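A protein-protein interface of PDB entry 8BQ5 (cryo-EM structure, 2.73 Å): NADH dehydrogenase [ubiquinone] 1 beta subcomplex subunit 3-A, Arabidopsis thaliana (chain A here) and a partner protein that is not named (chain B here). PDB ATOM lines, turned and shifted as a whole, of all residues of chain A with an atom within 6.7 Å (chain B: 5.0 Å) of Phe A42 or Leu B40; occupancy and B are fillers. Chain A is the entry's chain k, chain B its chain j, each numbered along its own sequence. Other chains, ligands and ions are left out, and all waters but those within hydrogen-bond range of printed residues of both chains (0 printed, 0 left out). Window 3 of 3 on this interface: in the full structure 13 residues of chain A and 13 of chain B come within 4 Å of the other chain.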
ATOM      1  N   ILE A  35       7.528 -11.967   3.337  1.00  0.00           N
ATOM      2  CA  ILE A  35       8.459 -11.237   4.193  1.00  0.00           C
ATOM      3  C   ILE A  35       9.902 -11.606   3.864  1.00  0.00           C
ATOM      4  O   ILE A  35      10.781 -10.737   3.844  1.00  0.00           O
ATOM      5  CB  ILE A  35       8.122 -11.475   5.680  1.00  0.00           C
ATOM      6  CG1 ILE A  35       8.993 -10.598   6.589  1.00  0.00           C
ATOM      7  CG2 ILE A  35       8.239 -12.948   6.052  1.00  0.00           C
ATOM      8  CD1 ILE A  35       8.590  -9.137   6.625  1.00  0.00           C
ATOM      9  N   ILE A  37      11.000 -12.792   0.897  1.00  0.00           N
ATOM     10  CA  ILE A  37      11.297 -12.254  -0.427  1.00  0.00           C
ATOM     11  C   ILE A  37      11.579 -10.762  -0.343  1.00  0.00           C
ATOM     12  O   ILE A  37      12.527 -10.257  -0.959  1.00  0.00           O
ATOM     13  CB  ILE A  37      10.138 -12.552  -1.398  1.00  0.00           C
ATOM     14  CG1 ILE A  37       9.448 -13.867  -1.027  1.00  0.00           C
ATOM     15  CG2 ILE A  37      10.643 -12.579  -2.832  1.00  0.00           C
ATOM     16  CD1 ILE A  37      10.267 -15.104  -1.333  1.00  0.00           C
ATOM     17  N   GLY A  38      10.763 -10.032   0.420  1.00  0.00           N
ATOM     18  CA  GLY A  38      10.924  -8.590   0.496  1.00  0.00           C
ATOM     19  C   GLY A  38      12.200  -8.171   1.198  1.00  0.00           C
ATOM     20  O   GLY A  38      12.844  -7.195   0.806  1.00  0.00           O
ATOM     21  N   VAL A  39      12.577  -8.894   2.254  1.00  0.00           N
ATOM     22  CA  VAL A  39      13.792  -8.561   2.989  1.00  0.00           C
ATOM     23  C   VAL A  39      15.024  -8.781   2.119  1.00  0.00           C
ATOM     24  O   VAL A  39      15.905  -7.918   2.036  1.00  0.00           O
ATOM     25  CB  VAL A  39      13.861  -9.378   4.293  1.00  0.00           C
ATOM     26  CG1 VAL A  39      15.272  -9.375   4.849  1.00  0.00           C
ATOM     27  CG2 VAL A  39      12.886  -8.823   5.317  1.00  0.00           C
ATOM     28  N   GLY A  40      15.100  -9.933   1.449  1.00  0.00           N
ATOM     29  CA  GLY A  40      16.241 -10.205   0.591  1.00  0.00           C
ATOM     30  C   GLY A  40      16.314  -9.274  -0.604  1.00  0.00           C
ATOM     31  O   GLY A  40      17.401  -8.876  -1.028  1.00  0.00           O
ATOM     32  N   ALA A  41      15.158  -8.921  -1.171  1.00  0.00           N
ATOM     33  CA  ALA A  41      15.141  -7.964  -2.271  1.00  0.00           C
ATOM     34  C   ALA A  41      15.685  -6.613  -1.827  1.00  0.00           C
ATOM     35  O   ALA A  41      16.255  -5.867  -2.630  1.00  0.00           O
ATOM     36  CB  ALA A  41      13.724  -7.820  -2.824  1.00  0.00           C
ATOM     37  N   PHE A  42      15.549  -6.309  -0.529  1.00  0.00           N
ATOM     38  CA  PHE A  42      16.083  -5.026  -0.004  1.00  0.00           C
ATOM     39  C   PHE A  42      17.596  -5.139   0.150  1.00  0.00           C
ATOM     40  O   PHE A  42      18.299  -4.159  -0.146  1.00  0.00           O
ATOM     41  CB  PHE A  42      15.465  -4.640   1.340  1.00  0.00           C
ATOM     42  CG  PHE A  42      15.733  -3.214   1.743  1.00  0.00           C
ATOM     43  CD1 PHE A  42      15.524  -2.176   0.849  1.00  0.00           C
ATOM     44  CD2 PHE A  42      16.211  -2.911   3.006  1.00  0.00           C
ATOM     45  CE1 PHE A  42      15.786  -0.866   1.214  1.00  0.00           C
ATOM     46  CE2 PHE A  42      16.463  -1.598   3.372  1.00  0.00           C
ATOM     47  CZ  PHE A  42      16.253  -0.580   2.474  1.00  0.00           C
ATOM     48  N   CYS A  43      18.063  -6.298   0.612  1.00  0.00           N
ATOM     49  CA  CYS A  43      19.500  -6.487   0.774  1.00  0.00           C
ATOM     50  C   CYS A  43      20.221  -6.421  -0.565  1.00  0.00           C
ATOM     51  O   CYS A  43      21.257  -5.760  -0.689  1.00  0.00           O
ATOM     52  CB  CYS A  43      19.778  -7.822   1.466  1.00  0.00           C
ATOM     53  SG  CYS A  43      19.291  -7.880   3.204  1.00  0.00           S
ATOM     54  N   VAL A  44      19.678  -7.093  -1.584  1.00  0.00           N
ATOM     55  CA  VAL A  44      20.307  -7.093  -2.903  1.00  0.00           C
ATOM     56  C   VAL A  44      20.347  -5.680  -3.470  1.00  0.00           C
ATOM     57  O   VAL A  44      21.325  -5.279  -4.114  1.00  0.00           O
ATOM     58  CB  VAL A  44      19.568  -8.066  -3.841  1.00  0.00           C
ATOM     59  CG1 VAL A  44      20.109  -7.966  -5.260  1.00  0.00           C
ATOM     60  CG2 VAL A  44      19.673  -9.490  -3.318  1.00  0.00           C
ATOM     61  N   TYR A  45      19.303  -4.899  -3.178  1.00  0.00           N
ATOM     62  CA  TYR A  45      19.298  -3.473  -3.586  1.00  0.00           C
ATOM     63  C   TYR A  45      20.357  -2.738  -2.765  1.00  0.00           C
ATOM     64  O   TYR A  45      21.051  -1.858  -3.310  1.00  0.00           O
ATOM     65  CB  TYR A  45      17.918  -2.858  -3.332  1.00  0.00           C
ATOM     66  CG  TYR A  45      17.914  -1.352  -3.283  1.00  0.00           C
ATOM     67  CD1 TYR A  45      18.116  -0.608  -4.434  1.00  0.00           C
ATOM     68  CD2 TYR A  45      17.744  -0.672  -2.089  1.00  0.00           C
ATOM     69  CE1 TYR A  45      18.143   0.774  -4.404  1.00  0.00           C
ATOM     70  CE2 TYR A  45      17.766   0.712  -2.043  1.00  0.00           C
ATOM     71  CZ  TYR A  45      17.967   1.437  -3.204  1.00  0.00           C
ATOM     72  OH  TYR A  45      17.992   2.799  -3.182  1.00  0.00           O
ATOM     73  N   LEU A  46      20.498  -3.106  -1.498  1.00  0.00           N
ATOM     74  CA  LEU A  46      21.414  -2.403  -0.606  1.00  0.00           C
ATOM     75  C   LEU A  46      22.864  -2.588  -1.039  1.00  0.00           C
ATOM     76  O   LEU A  46      23.662  -1.645  -0.983  1.00  0.00           O
ATOM     77  CB  LEU A  46      21.206  -2.891   0.825  1.00  0.00           C
ATOM     78  CG  LEU A  46      20.590  -1.887   1.798  1.00  0.00           C
ATOM     79  CD1 LEU A  46      20.389  -2.533   3.159  1.00  0.00           C
ATOM     80  CD2 LEU A  46      21.454  -0.640   1.906  1.00  0.00           C
ATOM     81  N   VAL A  47      23.227  -3.802  -1.462  1.00  0.00           N
ATOM     82  CA  VAL A  47      24.571  -4.036  -1.983  1.00  0.00           C
ATOM     83  C   VAL A  47      24.768  -3.295  -3.299  1.00  0.00           C
ATOM     84  O   VAL A  47      25.856  -2.780  -3.583  1.00  0.00           O
ATOM     85  CB  VAL A  47      24.830  -5.546  -2.136  1.00  0.00           C
ATOM     86  CG1 VAL A  47      26.307  -5.811  -2.394  1.00  0.00           C
ATOM     87  CG2 VAL A  47      24.369  -6.289  -0.896  1.00  0.00           C
ATOM     88  N   TRP B  36       6.570  -4.867   1.655  1.00  0.00           N
ATOM     89  CA  TRP B  36       7.671  -4.895   2.615  1.00  0.00           C
ATOM     90  C   TRP B  36       8.886  -4.157   2.072  1.00  0.00           C
ATOM     91  O   TRP B  36       9.515  -3.368   2.786  1.00  0.00           O
ATOM     92  CB  TRP B  36       8.043  -6.337   2.966  1.00  0.00           C
ATOM     93  CG  TRP B  36       6.919  -7.154   3.528  1.00  0.00           C
ATOM     94  CD1 TRP B  36       6.422  -8.317   3.021  1.00  0.00           C
ATOM     95  CD2 TRP B  36       6.166  -6.882   4.716  1.00  0.00           C
ATOM     96  NE1 TRP B  36       5.399  -8.780   3.807  1.00  0.00           N
ATOM     97  CE2 TRP B  36       5.222  -7.919   4.857  1.00  0.00           C
ATOM     98  CE3 TRP B  36       6.194  -5.861   5.671  1.00  0.00           C
ATOM     99  CZ2 TRP B  36       4.316  -7.964   5.913  1.00  0.00           C
ATOM    100  CZ3 TRP B  36       5.293  -5.908   6.717  1.00  0.00           C
ATOM    101  CH2 TRP B  36       4.368  -6.952   6.830  1.00  0.00           C
ATOM    102  N   PHE B  37       9.226  -4.395   0.802  1.00  0.00           N
ATOM    103  CA  PHE B  37      10.329  -3.676   0.176  1.00  0.00           C
ATOM    104  C   PHE B  37      10.044  -2.180   0.106  1.00  0.00           C
ATOM    105  O   PHE B  37      10.963  -1.362   0.225  1.00  0.00           O
ATOM    106  CB  PHE B  37      10.590  -4.247  -1.218  1.00  0.00           C
ATOM    107  CG  PHE B  37      11.697  -3.561  -1.963  1.00  0.00           C
ATOM    108  CD1 PHE B  37      13.002  -4.014  -1.863  1.00  0.00           C
ATOM    109  CD2 PHE B  37      11.431  -2.480  -2.788  1.00  0.00           C
ATOM    110  CE1 PHE B  37      14.019  -3.391  -2.554  1.00  0.00           C
ATOM    111  CE2 PHE B  37      12.444  -1.854  -3.478  1.00  0.00           C
ATOM    112  CZ  PHE B  37      13.739  -2.310  -3.363  1.00  0.00           C
ATOM    113  N   TRP B  38       8.779  -1.807  -0.104  1.00  0.00           N
ATOM    114  CA  TRP B  38       8.410  -0.395  -0.089  1.00  0.00           C
ATOM    115  C   TRP B  38       8.650   0.225   1.280  1.00  0.00           C
ATOM    116  O   TRP B  38       9.183   1.337   1.384  1.00  0.00           O
ATOM    117  CB  TRP B  38       6.945  -0.243  -0.497  1.00  0.00           C
ATOM    118  CG  TRP B  38       6.431   1.165  -0.475  1.00  0.00           C
ATOM    119  CD1 TRP B  38       5.523   1.688   0.396  1.00  0.00           C
ATOM    120  CD2 TRP B  38       6.773   2.223  -1.379  1.00  0.00           C
ATOM    121  NE1 TRP B  38       5.285   3.006   0.102  1.00  0.00           N
ATOM    122  CE2 TRP B  38       6.041   3.360  -0.986  1.00  0.00           C
ATOM    123  CE3 TRP B  38       7.631   2.321  -2.477  1.00  0.00           C
ATOM    124  CZ2 TRP B  38       6.140   4.579  -1.651  1.00  0.00           C
ATOM    125  CZ3 TRP B  38       7.728   3.533  -3.137  1.00  0.00           C
ATOM    126  CH2 TRP B  38       6.988   4.645  -2.722  1.00  0.00           C
ATOM    127  N   ILE B  39       8.273  -0.483   2.345  1.00  0.00           N
ATOM    128  CA  ILE B  39       8.379   0.078   3.689  1.00  0.00           C
ATOM    129  C   ILE B  39       9.839   0.204   4.105  1.00  0.00           C
ATOM    130  O   ILE B  39      10.244   1.207   4.704  1.00  0.00           O
ATOM    131  CB  ILE B  39       7.566  -0.772   4.682  1.00  0.00           C
ATOM    132  CG1 ILE B  39       6.070  -0.591   4.419  1.00  0.00           C
ATOM    133  CG2 ILE B  39       7.896  -0.398   6.115  1.00  0.00           C
ATOM    134  CD1 ILE B  39       5.200  -1.595   5.132  1.00  0.00           C
ATOM    135  N   LEU B  40      10.632  -0.838   3.850  1.00  0.00           N
ATOM    136  CA  LEU B  40      12.064  -0.823   4.265  1.00  0.00           C
ATOM    137  C   LEU B  40      12.782   0.312   3.530  1.00  0.00           C
ATOM    138  O   LEU B  40      13.559   1.013   4.183  1.00  0.00           O
ATOM    139  CB  LEU B  40      12.694  -2.180   3.950  1.00  0.00           C
ATOM    140  CG  LEU B  40      12.212  -3.348   4.806  1.00  0.00           C
ATOM    141  CD1 LEU B  40      12.833  -4.656   4.341  1.00  0.00           C
ATOM    142  CD2 LEU B  40      12.505  -3.106   6.278  1.00  0.00           C
ATOM    143  N   TYR B  41      12.499   0.489   2.237  1.00  0.00           N
ATOM    144  CA  TYR B  41      13.093   1.586   1.431  1.00  0.00           C
ATOM    145  C   TYR B  41      12.663   2.958   1.966  1.00  0.00           C
ATOM    146  O   TYR B  41      13.523   3.825   2.063  1.00  0.00           O
ATOM    147  CB  TYR B  41      12.696   1.414  -0.034  1.00  0.00           C
ATOM    148  CG  TYR B  41      13.225   2.471  -0.965  1.00  0.00           C
ATOM    149  CD1 TYR B  41      12.404   3.479  -1.442  1.00  0.00           C
ATOM    150  CD2 TYR B  41      14.548   2.462  -1.371  1.00  0.00           C
ATOM    151  CE1 TYR B  41      12.884   4.454  -2.298  1.00  0.00           C
ATOM    152  CE2 TYR B  41      15.041   3.429  -2.228  1.00  0.00           C
ATOM    153  CZ  TYR B  41      14.208   4.428  -2.695  1.00  0.00           C
ATOM    154  OH  TYR B  41      14.692   5.383  -3.540  1.00  0.00           O
ATOM    155  N   ARG B  42      11.369   3.153   2.233  1.00  0.00           N
ATOM    156  CA  ARG B  42      10.888   4.481   2.693  1.00  0.00           C
ATOM    157  C   ARG B  42      11.395   4.711   4.120  1.00  0.00           C
ATOM    158  O   ARG B  42      11.646   5.864   4.458  1.00  0.00           O
ATOM    159  CB  ARG B  42       9.368   4.611   2.580  1.00  0.00           C
ATOM    160  CG  ARG B  42       8.857   4.712   1.151  1.00  0.00           C
ATOM    161  CD  ARG B  42       8.468   6.128   0.776  1.00  0.00           C
ATOM    162  NE  ARG B  42       9.631   6.978   0.574  1.00  0.00           N
ATOM    163  CZ  ARG B  42      10.279   7.119  -0.577  1.00  0.00           C
ATOM    164  NH1 ARG B  42       9.875   6.470  -1.656  1.00  0.00           N
ATOM    165  NH2 ARG B  42      11.330   7.916  -0.644  1.00  0.00           N
ATOM    166  N   ALA B  43      11.567   3.651   4.912  1.00  0.00           N
ATOM    167  CA  ALA B  43      12.176   3.822   6.251  1.00  0.00           C
ATOM    168  C   ALA B  43      13.646   4.218   6.073  1.00  0.00           C
ATOM    169  O   ALA B  43      14.135   5.012   6.880  1.00  0.00           O
ATOM    170  CB  ALA B  43      12.037   2.558   7.054  1.00  0.00           C
ATOM    171  N   LYS B  44      14.319   3.684   5.045  1.00  0.00           N
ATOM    172  CA  LYS B  44      15.719   4.086   4.755  1.00  0.00           C
ATOM    173  C   LYS B  44      15.786   5.589   4.475  1.00  0.00           C
ATOM    174  O   LYS B  44      16.695   6.233   5.030  1.00  0.00           O
ATOM    175  CB  LYS B  44      16.274   3.346   3.535  1.00  0.00           C
ATOM    176  CG  LYS B  44      17.792   3.236   3.469  1.00  0.00           C
ATOM    177  CD  LYS B  44      18.374   3.778   2.181  1.00  0.00           C
ATOM    178  CE  LYS B  44      18.183   2.846   1.004  1.00  0.00           C
ATOM    179  NZ  LYS B  44      18.747   3.417  -0.241  1.00  0.00           N
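Of the 12 printed residues of chain A, 4 touch a printed residue of chain B. Hydrophobic or aromatic side chains of chain A that line the printed part of chain B: Ile A35, Ala A41, Phe A42 and Tyr A45. Among the printed residues, no Asp or Glu carboxylate lies within 4 Å of a Lys or Arg side-chain nitrogen of the other chain.
Ile A35 touches Trp B36 (CA to CD1, 3.7 Å). Phe B37 touches Ala A41 (CE1 to O, 3.3 Å). CA of Phe A42 touches CE1 of Phe B37, 3.7 Å away. CZ of Phe A42 touches O of Leu B40, 3.6 Å away. CE1 of Phe A42 touches CA of Tyr B41 (3.6 Å). Tyr A45 touches Tyr B41 (OH to CE2, 3.2 Å).
Of the printed residues of chain B, Ala A41 touches Phe B37. Printed residues of chain B within 4 Å of Phe A42: Phe B37, Leu B40 and Tyr B41. Of the printed residues of chain B, Tyr A45 touches Tyr B41 (3.2 Å) and Lys B44 (3.1 Å). Val A47 touches none of the printed residues of chain B. Of the printed residues of chain A, Trp B36 touches Ile A35. Printed residues of chain A within 4 Å of Phe B37: Ala A41 and Phe A42. Leu B40 touches just one residue of chain A: Phe A42. Of the printed residues of chain A, Tyr B41 touches Phe A42 (3.6 Å) and Tyr A45 (3.2 Å). The nearest residue of chain B that does not touch Phe A42 is Lys B44 (4.1 Å).
NZ of Lys B44 lies within hydrogen-bond range of OH of Tyr A45, 3.1 Å away.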
